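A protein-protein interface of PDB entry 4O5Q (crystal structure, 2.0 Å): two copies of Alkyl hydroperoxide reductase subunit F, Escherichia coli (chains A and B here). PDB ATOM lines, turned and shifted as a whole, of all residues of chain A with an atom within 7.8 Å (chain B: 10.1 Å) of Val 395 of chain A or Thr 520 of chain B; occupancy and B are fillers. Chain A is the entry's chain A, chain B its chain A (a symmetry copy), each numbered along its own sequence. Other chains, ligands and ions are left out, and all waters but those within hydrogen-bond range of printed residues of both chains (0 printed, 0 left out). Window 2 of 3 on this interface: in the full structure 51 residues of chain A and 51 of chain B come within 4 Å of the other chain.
OD2 of Asp 393 of chain A lies within salt-bridge range of NH2 of Arg 517 of chain B (2.9 Å).
The side-chain amide oxygen (OD1) of Asn 365 of chain A sits at hydrogen-bond distance from the backbone NH (N) of Asp 393 of chain A, at 2.8 Å.
O of Lys 399 of chain A sits at hydrogen-bond distance from OG of Ser 402 of chain A (2.8 Å).
The guanidinium group of Arg 517 of chain B is in salt-bridge range of the side-chain carboxylate of Asp 513 of chain B (3.0 Å).
Ile 372 of chain A touches Ile 516 of chain B (CD1 to CG2, 3.9 Å).
Val 395 of chain A touches Arg 517 of chain B (CG1 to NH1, 3.8 Å).
Val 395 of chain A touches Thr 520 of chain B (CG2 to CG2, 3.98 Å).
CD2 of Leu 396 of chain A touches CG2 of Ile 516 of chain B, at 3.6 Å.
Arg 517 of chain B touches Leu 396 of chain A (NH2 to CD1, 3.6 Å).
Lys 519 of chain B touches Lys 399 of chain A.
Of the printed residues of chain B, Asp 393 of chain A touches Arg 517 (2.9 Å).
No residue of chain B comes within 4 Å of Gln 394 of chain A.
Of the printed residues of chain B, Val 395 of chain A touches Arg 517 and Thr 520.
Of chain B, only Ile 516 (3.6 Å) and Arg 517 (3.6 Å) come within 4 Å of Leu 396 of chain A.
Printed residues of chain A within 4 Å of Ile 516 of chain B: Ile 372 and Leu 396.
Of the printed residues of chain A, Arg 517 of chain B touches Asp 393 (2.9 Å), Val 395 (3.8 Å) and Leu 396 (3.6 Å).
Of the printed residues of chain A, Thr 520 of chain B touches Val 395.
The nearest printed residue of chain A that does not touch Thr 520 of chain B is Lys 399 of chain A (5.7 Å).
Printed residues of chain B that touch a printed residue of chain A: Ile 516, Arg 517, Lys 519 and Thr 520.
Hydrophobic or aromatic side chains of chain B that line the printed part of chain A: Ile 516.
Of the 14 printed residues of chain A, 5 touch a printed residue of chain B.
Printed residues of chain A that touch a printed residue of chain B: Ile 372, Asp 393, Val 395, Leu 396 and Lys 399.
Hydrophobic or aromatic side chains of chain A within 4 Å of the printed part of chain B: Ile 372, Val 395 and Leu 396.
No position is printed for both chains.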
ATOM      1  N   ASN A 365       5.060  20.974  18.474  1.00  0.00           N
ATOM      2  CA  ASN A 365       5.784  19.977  19.245  1.00  0.00           C
ATOM      3  C   ASN A 365       6.853  20.570  20.103  1.00  0.00           C
ATOM      4  O   ASN A 365       7.030  20.173  21.252  1.00  0.00           O
ATOM      5  CB  ASN A 365       6.454  18.921  18.324  1.00  0.00           C
ATOM      6  CG  ASN A 365       5.472  17.852  17.842  1.00  0.00           C
ATOM      7  OD1 ASN A 365       4.369  17.697  18.386  1.00  0.00           O
ATOM      8  ND2 ASN A 365       5.882  17.090  16.827  1.00  0.00           N
ATOM      9  N   VAL A 368       5.234  22.575  23.084  1.00  0.00           N
ATOM     10  CA  VAL A 368       4.634  21.651  24.048  1.00  0.00           C
ATOM     11  C   VAL A 368       5.686  20.817  24.753  1.00  0.00           C
ATOM     12  O   VAL A 368       5.648  20.668  25.968  1.00  0.00           O
ATOM     13  CB  VAL A 368       3.558  20.770  23.397  1.00  0.00           C
ATOM     14  CG1 VAL A 368       3.061  19.693  24.374  1.00  0.00           C
ATOM     15  CG2 VAL A 368       2.382  21.645  22.978  1.00  0.00           C
ATOM     16  N   ILE A 372       6.688  20.773  28.779  1.00  0.00           N
ATOM     17  CA  ILE A 372       6.747  19.580  29.615  1.00  0.00           C
ATOM     18  C   ILE A 372       8.149  19.516  30.262  1.00  0.00           C
ATOM     19  O   ILE A 372       8.292  19.312  31.464  1.00  0.00           O
ATOM     20  CB  ILE A 372       6.501  18.307  28.777  1.00  0.00           C
ATOM     21  CG1 ILE A 372       5.061  18.274  28.278  1.00  0.00           C
ATOM     22  CG2 ILE A 372       6.778  17.010  29.610  1.00  0.00           C
ATOM     23  CD1 ILE A 372       4.796  17.216  27.193  1.00  0.00           C
ATOM     24  N   ALA A 392       0.668  20.350  18.467  1.00  0.00           N
ATOM     25  CA  ALA A 392       1.549  19.253  18.855  1.00  0.00           C
ATOM     26  C   ALA A 392       0.881  17.869  18.751  1.00  0.00           C
ATOM     27  O   ALA A 392      -0.346  17.766  18.832  1.00  0.00           O
ATOM     28  CB  ALA A 392       2.029  19.489  20.266  1.00  0.00           C
ATOM     29  N   ASP A 393       1.707  16.815  18.636  1.00  0.00           N
ATOM     30  CA  ASP A 393       1.237  15.428  18.710  1.00  0.00           C
ATOM     31  C   ASP A 393       0.354  15.231  19.903  1.00  0.00           C
ATOM     32  O   ASP A 393       0.616  15.751  20.993  1.00  0.00           O
ATOM     33  CB  ASP A 393       2.396  14.428  18.879  1.00  0.00           C
ATOM     34  CG  ASP A 393       3.376  14.453  17.737  1.00  0.00           C
ATOM     35  OD1 ASP A 393       3.028  14.937  16.642  1.00  0.00           O
ATOM     36  OD2 ASP A 393       4.506  13.963  17.939  1.00  0.00           O
ATOM     37  N   GLN A 394      -0.656  14.398  19.730  1.00  0.00           N
ATOM     38  CA  GLN A 394      -1.647  14.204  20.776  1.00  0.00           C
ATOM     39  C   GLN A 394      -1.028  13.676  22.071  1.00  0.00           C
ATOM     40  O   GLN A 394      -1.460  14.048  23.149  1.00  0.00           O
ATOM     41  CB  GLN A 394      -2.726  13.224  20.309  1.00  0.00           C
ATOM     42  CG  GLN A 394      -3.897  13.150  21.270  1.00  0.00           C
ATOM     43  CD  GLN A 394      -4.697  14.434  21.292  1.00  0.00           C
ATOM     44  OE1 GLN A 394      -4.904  15.062  20.252  1.00  0.00           O
ATOM     45  NE2 GLN A 394      -5.141  14.843  22.477  1.00  0.00           N
ATOM     46  N   VAL A 395      -0.015  12.819  21.969  1.00  0.00           N
ATOM     47  CA  VAL A 395       0.601  12.269  23.174  1.00  0.00           C
ATOM     48  C   VAL A 395       1.226  13.381  24.024  1.00  0.00           C
ATOM     49  O   VAL A 395       1.162  13.351  25.252  1.00  0.00           O
ATOM     50  CB  VAL A 395       1.660  11.146  22.847  1.00  0.00           C
ATOM     51  CG1 VAL A 395       2.854  11.695  22.092  1.00  0.00           C
ATOM     52  CG2 VAL A 395       2.109  10.461  24.107  1.00  0.00           C
ATOM     53  N   LEU A 396       1.855  14.340  23.365  1.00  0.00           N
ATOM     54  CA  LEU A 396       2.446  15.467  24.050  1.00  0.00           C
ATOM     55  C   LEU A 396       1.369  16.347  24.681  1.00  0.00           C
ATOM     56  O   LEU A 396       1.504  16.790  25.834  1.00  0.00           O
ATOM     57  CB  LEU A 396       3.302  16.266  23.057  1.00  0.00           C
ATOM     58  CG  LEU A 396       4.540  15.544  22.506  1.00  0.00           C
ATOM     59  CD1 LEU A 396       5.312  16.412  21.532  1.00  0.00           C
ATOM     60  CD2 LEU A 396       5.467  15.134  23.627  1.00  0.00           C
ATOM     61  N   GLN A 397       0.283  16.593  23.947  1.00  0.00           N
ATOM     62  CA  GLN A 397      -0.771  17.459  24.478  1.00  0.00           C
ATOM     63  C   GLN A 397      -1.349  16.804  25.703  1.00  0.00           C
ATOM     64  O   GLN A 397      -1.599  17.461  26.712  1.00  0.00           O
ATOM     65  CB  GLN A 397      -1.912  17.674  23.472  1.00  0.00           C
ATOM     66  CG  GLN A 397      -1.533  18.357  22.197  1.00  0.00           C
ATOM     67  CD  GLN A 397      -2.754  18.832  21.410  1.00  0.00           C
ATOM     68  OE1 GLN A 397      -3.785  19.164  21.989  1.00  0.00           O
ATOM     69  NE2 GLN A 397      -2.633  18.868  20.096  1.00  0.00           N
ATOM     70  N   ASP A 398      -1.599  15.501  25.617  1.00  0.00           N
ATOM     71  CA  ASP A 398      -2.153  14.773  26.771  1.00  0.00           C
ATOM     72  C   ASP A 398      -1.172  14.827  27.952  1.00  0.00           C
ATOM     73  O   ASP A 398      -1.559  15.022  29.100  1.00  0.00           O
ATOM     74  CB  ASP A 398      -2.430  13.301  26.418  1.00  0.00           C
ATOM     75  CG  ASP A 398      -3.586  13.128  25.426  1.00  0.00           C
ATOM     76  OD1 ASP A 398      -4.434  14.040  25.314  1.00  0.00           O
ATOM     77  OD2 ASP A 398      -3.639  12.065  24.762  1.00  0.00           O
ATOM     78  N   LYS A 399       0.108  14.650  27.660  1.00  0.00           N
ATOM     79  CA  LYS A 399       1.072  14.710  28.739  1.00  0.00           C
ATOM     80  C   LYS A 399       1.062  16.117  29.389  1.00  0.00           C
ATOM     81  O   LYS A 399       1.004  16.255  30.614  1.00  0.00           O
ATOM     82  CB  LYS A 399       2.458  14.314  28.256  1.00  0.00           C
ATOM     83  CG  LYS A 399       3.487  14.263  29.389  1.00  0.00           C
ATOM     84  CD  LYS A 399       2.859  13.769  30.704  1.00  0.00           C
ATOM     85  CE  LYS A 399       3.817  13.850  31.837  1.00  0.00           C
ATOM     86  NZ  LYS A 399       4.672  12.681  31.739  1.00  0.00           N
ATOM     87  N   LEU A 400       1.040  17.164  28.575  1.00  0.00           N
ATOM     88  CA  LEU A 400       1.055  18.527  29.131  1.00  0.00           C
ATOM     89  C   LEU A 400      -0.172  18.849  29.994  1.00  0.00           C
ATOM     90  O   LEU A 400      -0.054  19.462  31.062  1.00  0.00           O
ATOM     91  CB  LEU A 400       1.201  19.564  27.998  1.00  0.00           C
ATOM     92  CG  LEU A 400       1.459  21.015  28.447  1.00  0.00           C
ATOM     93  CD1 LEU A 400       2.757  21.139  29.227  1.00  0.00           C
ATOM     94  CD2 LEU A 400       1.518  21.988  27.253  1.00  0.00           C
ATOM     95  N   ARG A 401      -1.349  18.470  29.510  1.00  0.00           N
ATOM     96  CA  ARG A 401      -2.598  18.750  30.220  1.00  0.00           C
ATOM     97  C   ARG A 401      -2.715  17.961  31.546  1.00  0.00           C
ATOM     98  O   ARG A 401      -3.618  18.217  32.331  1.00  0.00           O
ATOM     99  CB  ARG A 401      -3.806  18.383  29.355  1.00  0.00           C
ATOM    100  CG  ARG A 401      -4.022  19.221  28.115  1.00  0.00           C
ATOM    101  CD  ARG A 401      -5.259  18.749  27.337  1.00  0.00           C
ATOM    102  NE  ARG A 401      -5.528  19.543  26.131  1.00  0.00           N
ATOM    103  CZ  ARG A 401      -5.976  20.802  26.149  1.00  0.00           C
ATOM    104  NH1 ARG A 401      -6.180  21.419  27.312  1.00  0.00           N
ATOM    105  NH2 ARG A 401      -6.204  21.455  25.008  1.00  0.00           N
ATOM    106  N   SER A 402      -1.826  17.002  31.770  1.00  0.00           N
ATOM    107  CA  SER A 402      -1.822  16.247  33.021  1.00  0.00           C
ATOM    108  C   SER A 402      -0.860  16.811  34.079  1.00  0.00           C
ATOM    109  O   SER A 402      -0.845  16.328  35.207  1.00  0.00           O
ATOM    110  CB  SER A 402      -1.470  14.783  32.758  1.00  0.00           C
ATOM    111  OG  SER A 402      -0.072  14.601  32.623  1.00  0.00           O
ATOM    112  N   VAL B 298       9.149  -4.264  28.120  1.00  0.00           N
ATOM    113  CA  VAL B 298       7.984  -3.505  27.707  1.00  0.00           C
ATOM    114  C   VAL B 298       8.380  -2.041  27.571  1.00  0.00           C
ATOM    115  O   VAL B 298       9.276  -1.556  28.287  1.00  0.00           O
ATOM    116  CB  VAL B 298       6.822  -3.664  28.773  1.00  0.00           C
ATOM    117  CG1 VAL B 298       7.179  -3.010  30.089  1.00  0.00           C
ATOM    118  CG2 VAL B 298       5.507  -3.111  28.262  1.00  0.00           C
ATOM    119  N   GLU B 299       7.728  -1.324  26.663  1.00  0.00           N
ATOM    120  CA  GLU B 299       7.889   0.130  26.556  1.00  0.00           C
ATOM    121  C   GLU B 299       7.516   0.790  27.870  1.00  0.00           C
ATOM    122  O   GLU B 299       6.474   0.487  28.430  1.00  0.00           O
ATOM    123  CB  GLU B 299       6.998   0.714  25.450  1.00  0.00           C
ATOM    124  CG  GLU B 299       6.860   2.243  25.520  1.00  0.00           C
ATOM    125  CD  GLU B 299       6.005   2.820  24.408  1.00  0.00           C
ATOM    126  OE1 GLU B 299       6.179   2.389  23.245  1.00  0.00           O
ATOM    127  OE2 GLU B 299       5.165   3.703  24.700  1.00  0.00           O
ATOM    128  N   GLY B 300       8.351   1.705  28.341  1.00  0.00           N
ATOM    129  CA  GLY B 300       8.120   2.344  29.613  1.00  0.00           C
ATOM    130  C   GLY B 300       8.608   1.488  30.770  1.00  0.00           C
ATOM    131  O   GLY B 300       8.358   1.808  31.918  1.00  0.00           O
ATOM    132  N   GLY B 301       9.267   0.374  30.459  1.00  0.00           N
ATOM    133  CA  GLY B 301       9.862  -0.475  31.474  1.00  0.00           C
ATOM    134  C   GLY B 301      11.212   0.059  31.852  1.00  0.00           C
ATOM    135  O   GLY B 301      11.464   1.274  31.806  1.00  0.00           O
ATOM    136  N   ARG B 316      15.518   3.942  32.784  1.00  0.00           N
ATOM    137  CA  ARG B 316      14.465   4.084  31.798  1.00  0.00           C
ATOM    138  C   ARG B 316      15.009   4.284  30.382  1.00  0.00           C
ATOM    139  O   ARG B 316      14.321   4.036  29.402  1.00  0.00           O
ATOM    140  CB  ARG B 316      13.675   5.336  32.080  1.00  0.00           C
ATOM    141  CG  ARG B 316      13.086   5.407  33.433  1.00  0.00           C
ATOM    142  CD  ARG B 316      11.750   5.957  33.141  1.00  0.00           C
ATOM    143  NE  ARG B 316      11.168   6.689  34.198  1.00  0.00           N
ATOM    144  CZ  ARG B 316       9.865   6.897  34.269  1.00  0.00           C
ATOM    145  NH1 ARG B 316       9.043   6.383  33.354  1.00  0.00           N
ATOM    146  NH2 ARG B 316       9.399   7.604  35.264  1.00  0.00           N
ATOM    147  N   ASP B 513      13.567  13.314  25.007  1.00  0.00           N
ATOM    148  CA  ASP B 513      12.351  13.231  24.186  1.00  0.00           C
ATOM    149  C   ASP B 513      11.649  11.874  24.353  1.00  0.00           C
ATOM    150  O   ASP B 513      10.417  11.809  24.485  1.00  0.00           O
ATOM    151  CB  ASP B 513      12.694  13.430  22.702  1.00  0.00           C
ATOM    152  CG  ASP B 513      11.511  13.096  21.784  1.00  0.00           C
ATOM    153  OD1 ASP B 513      10.592  13.913  21.732  1.00  0.00           O
ATOM    154  OD2 ASP B 513      11.467  12.011  21.157  1.00  0.00           O
ATOM    155  N   TYR B 514      12.431  10.792  24.360  1.00  0.00           N
ATOM    156  CA  TYR B 514      11.900   9.457  24.578  1.00  0.00           C
ATOM    157  C   TYR B 514      11.233   9.332  25.937  1.00  0.00           C
ATOM    158  O   TYR B 514      10.146   8.765  26.066  1.00  0.00           O
ATOM    159  CB  TYR B 514      13.031   8.397  24.491  1.00  0.00           C
ATOM    160  CG  TYR B 514      12.527   6.996  24.731  1.00  0.00           C
ATOM    161  CD1 TYR B 514      11.965   6.278  23.698  1.00  0.00           C
ATOM    162  CD2 TYR B 514      12.592   6.395  26.005  1.00  0.00           C
ATOM    163  CE1 TYR B 514      11.489   5.038  23.892  1.00  0.00           C
ATOM    164  CE2 TYR B 514      12.105   5.135  26.205  1.00  0.00           C
ATOM    165  CZ  TYR B 514      11.553   4.460  25.137  1.00  0.00           C
ATOM    166  OH  TYR B 514      11.066   3.178  25.259  1.00  0.00           O
ATOM    167  N   LEU B 515      11.859   9.903  26.960  1.00  0.00           N
ATOM    168  CA  LEU B 515      11.290   9.856  28.298  1.00  0.00           C
ATOM    169  C   LEU B 515       9.976  10.629  28.362  1.00  0.00           C
ATOM    170  O   LEU B 515       9.033  10.198  29.004  1.00  0.00           O
ATOM    171  CB  LEU B 515      12.230  10.453  29.326  1.00  0.00           C
ATOM    172  CG  LEU B 515      13.519   9.674  29.594  1.00  0.00           C
ATOM    173  CD1 LEU B 515      14.374  10.430  30.590  1.00  0.00           C
ATOM    174  CD2 LEU B 515      13.205   8.307  30.143  1.00  0.00           C
ATOM    175  N   ILE B 516       9.929  11.784  27.717  1.00  0.00           N
ATOM    176  CA  ILE B 516       8.698  12.574  27.670  1.00  0.00           C
ATOM    177  C   ILE B 516       7.595  11.766  27.010  1.00  0.00           C
ATOM    178  O   ILE B 516       6.470  11.719  27.494  1.00  0.00           O
ATOM    179  CB  ILE B 516       8.908  13.895  26.924  1.00  0.00           C
ATOM    180  CG1 ILE B 516       9.742  14.842  27.788  1.00  0.00           C
ATOM    181  CG2 ILE B 516       7.539  14.548  26.574  1.00  0.00           C
ATOM    182  CD1 ILE B 516      10.094  16.127  27.083  1.00  0.00           C
ATOM    183  N   ARG B 517       7.929  11.079  25.933  1.00  0.00           N
ATOM    184  CA  ARG B 517       6.925  10.351  25.171  1.00  0.00           C
ATOM    185  C   ARG B 517       6.538   8.954  25.697  1.00  0.00           C
ATOM    186  O   ARG B 517       5.632   8.348  25.160  1.00  0.00           O
ATOM    187  CB  ARG B 517       7.358  10.249  23.703  1.00  0.00           C
ATOM    188  CG  ARG B 517       7.378  11.576  22.963  1.00  0.00           C
ATOM    189  CD  ARG B 517       8.047  11.408  21.611  1.00  0.00           C
ATOM    190  NE  ARG B 517       8.013  12.639  20.833  1.00  0.00           N
ATOM    191  CZ  ARG B 517       6.985  13.008  20.061  1.00  0.00           C
ATOM    192  NH1 ARG B 517       5.905  12.244  19.956  1.00  0.00           N
ATOM    193  NH2 ARG B 517       7.043  14.130  19.374  1.00  0.00           N
ATOM    194  N   THR B 518       7.230   8.433  26.707  1.00  0.00           N
ATOM    195  CA  THR B 518       6.882   7.130  27.266  1.00  0.00           C
ATOM    196  C   THR B 518       6.404   7.253  28.695  1.00  0.00           C
ATOM    197  O   THR B 518       6.316   6.260  29.406  1.00  0.00           O
ATOM    198  CB  THR B 518       8.037   6.072  27.169  1.00  0.00           C
ATOM    199  OG1 THR B 518       9.229   6.582  27.777  1.00  0.00           O
ATOM    200  CG2 THR B 518       8.308   5.705  25.723  1.00  0.00           C
ATOM    201  N   LYS B 519       6.103   8.476  29.114  1.00  0.00           N
ATOM    202  CA  LYS B 519       5.343   8.675  30.337  1.00  0.00           C
ATOM    203  C   LYS B 519       3.863   8.722  29.978  1.00  0.00           C
ATOM    204  O   LYS B 519       3.145   9.663  30.329  1.00  0.00           O
ATOM    205  CB  LYS B 519       5.779   9.946  31.054  1.00  0.00           C
ATOM    206  CG  LYS B 519       7.094   9.765  31.759  1.00  0.00           C
ATOM    207  CD  LYS B 519       7.435  10.930  32.652  1.00  0.00           C
ATOM    208  CE  LYS B 519       8.586  10.563  33.547  1.00  0.00           C
ATOM    209  NZ  LYS B 519       9.683   9.931  32.761  1.00  0.00           N
ATOM    210  N   THR B 520       3.407   7.697  29.268  1.00  0.00           N
ATOM    211  CA  THR B 520       2.028   7.686  28.790  1.00  0.00           C
ATOM    212  C   THR B 520       1.015   7.439  29.922  1.00  0.00           C
ATOM    213  O   THR B 520      -0.204   7.358  29.686  1.00  0.00           O
ATOM    214  CB  THR B 520       1.850   6.692  27.624  1.00  0.00           C
ATOM    215  OG1 THR B 520       2.389   5.410  27.984  1.00  0.00           O
ATOM    216  CG2 THR B 520       2.563   7.227  26.382  1.00  0.00           C
ATOM    217  N   ALA B 521       1.543   7.324  31.140  1.00  0.00           N
ATOM    218  CA  ALA B 521       0.742   7.373  32.354  1.00  0.00           C
ATOM    219  C   ALA B 521       0.766   8.796  32.920  1.00  0.00           C
ATOM    220  O   ALA B 521       1.110   9.761  32.222  1.00  0.00           O
ATOM    221  CB  ALA B 521       1.274   6.387  33.374  1.00  0.00           C
ATOM    222  OXT ALA B 521       0.438   9.024  34.090  1.00  0.00           O
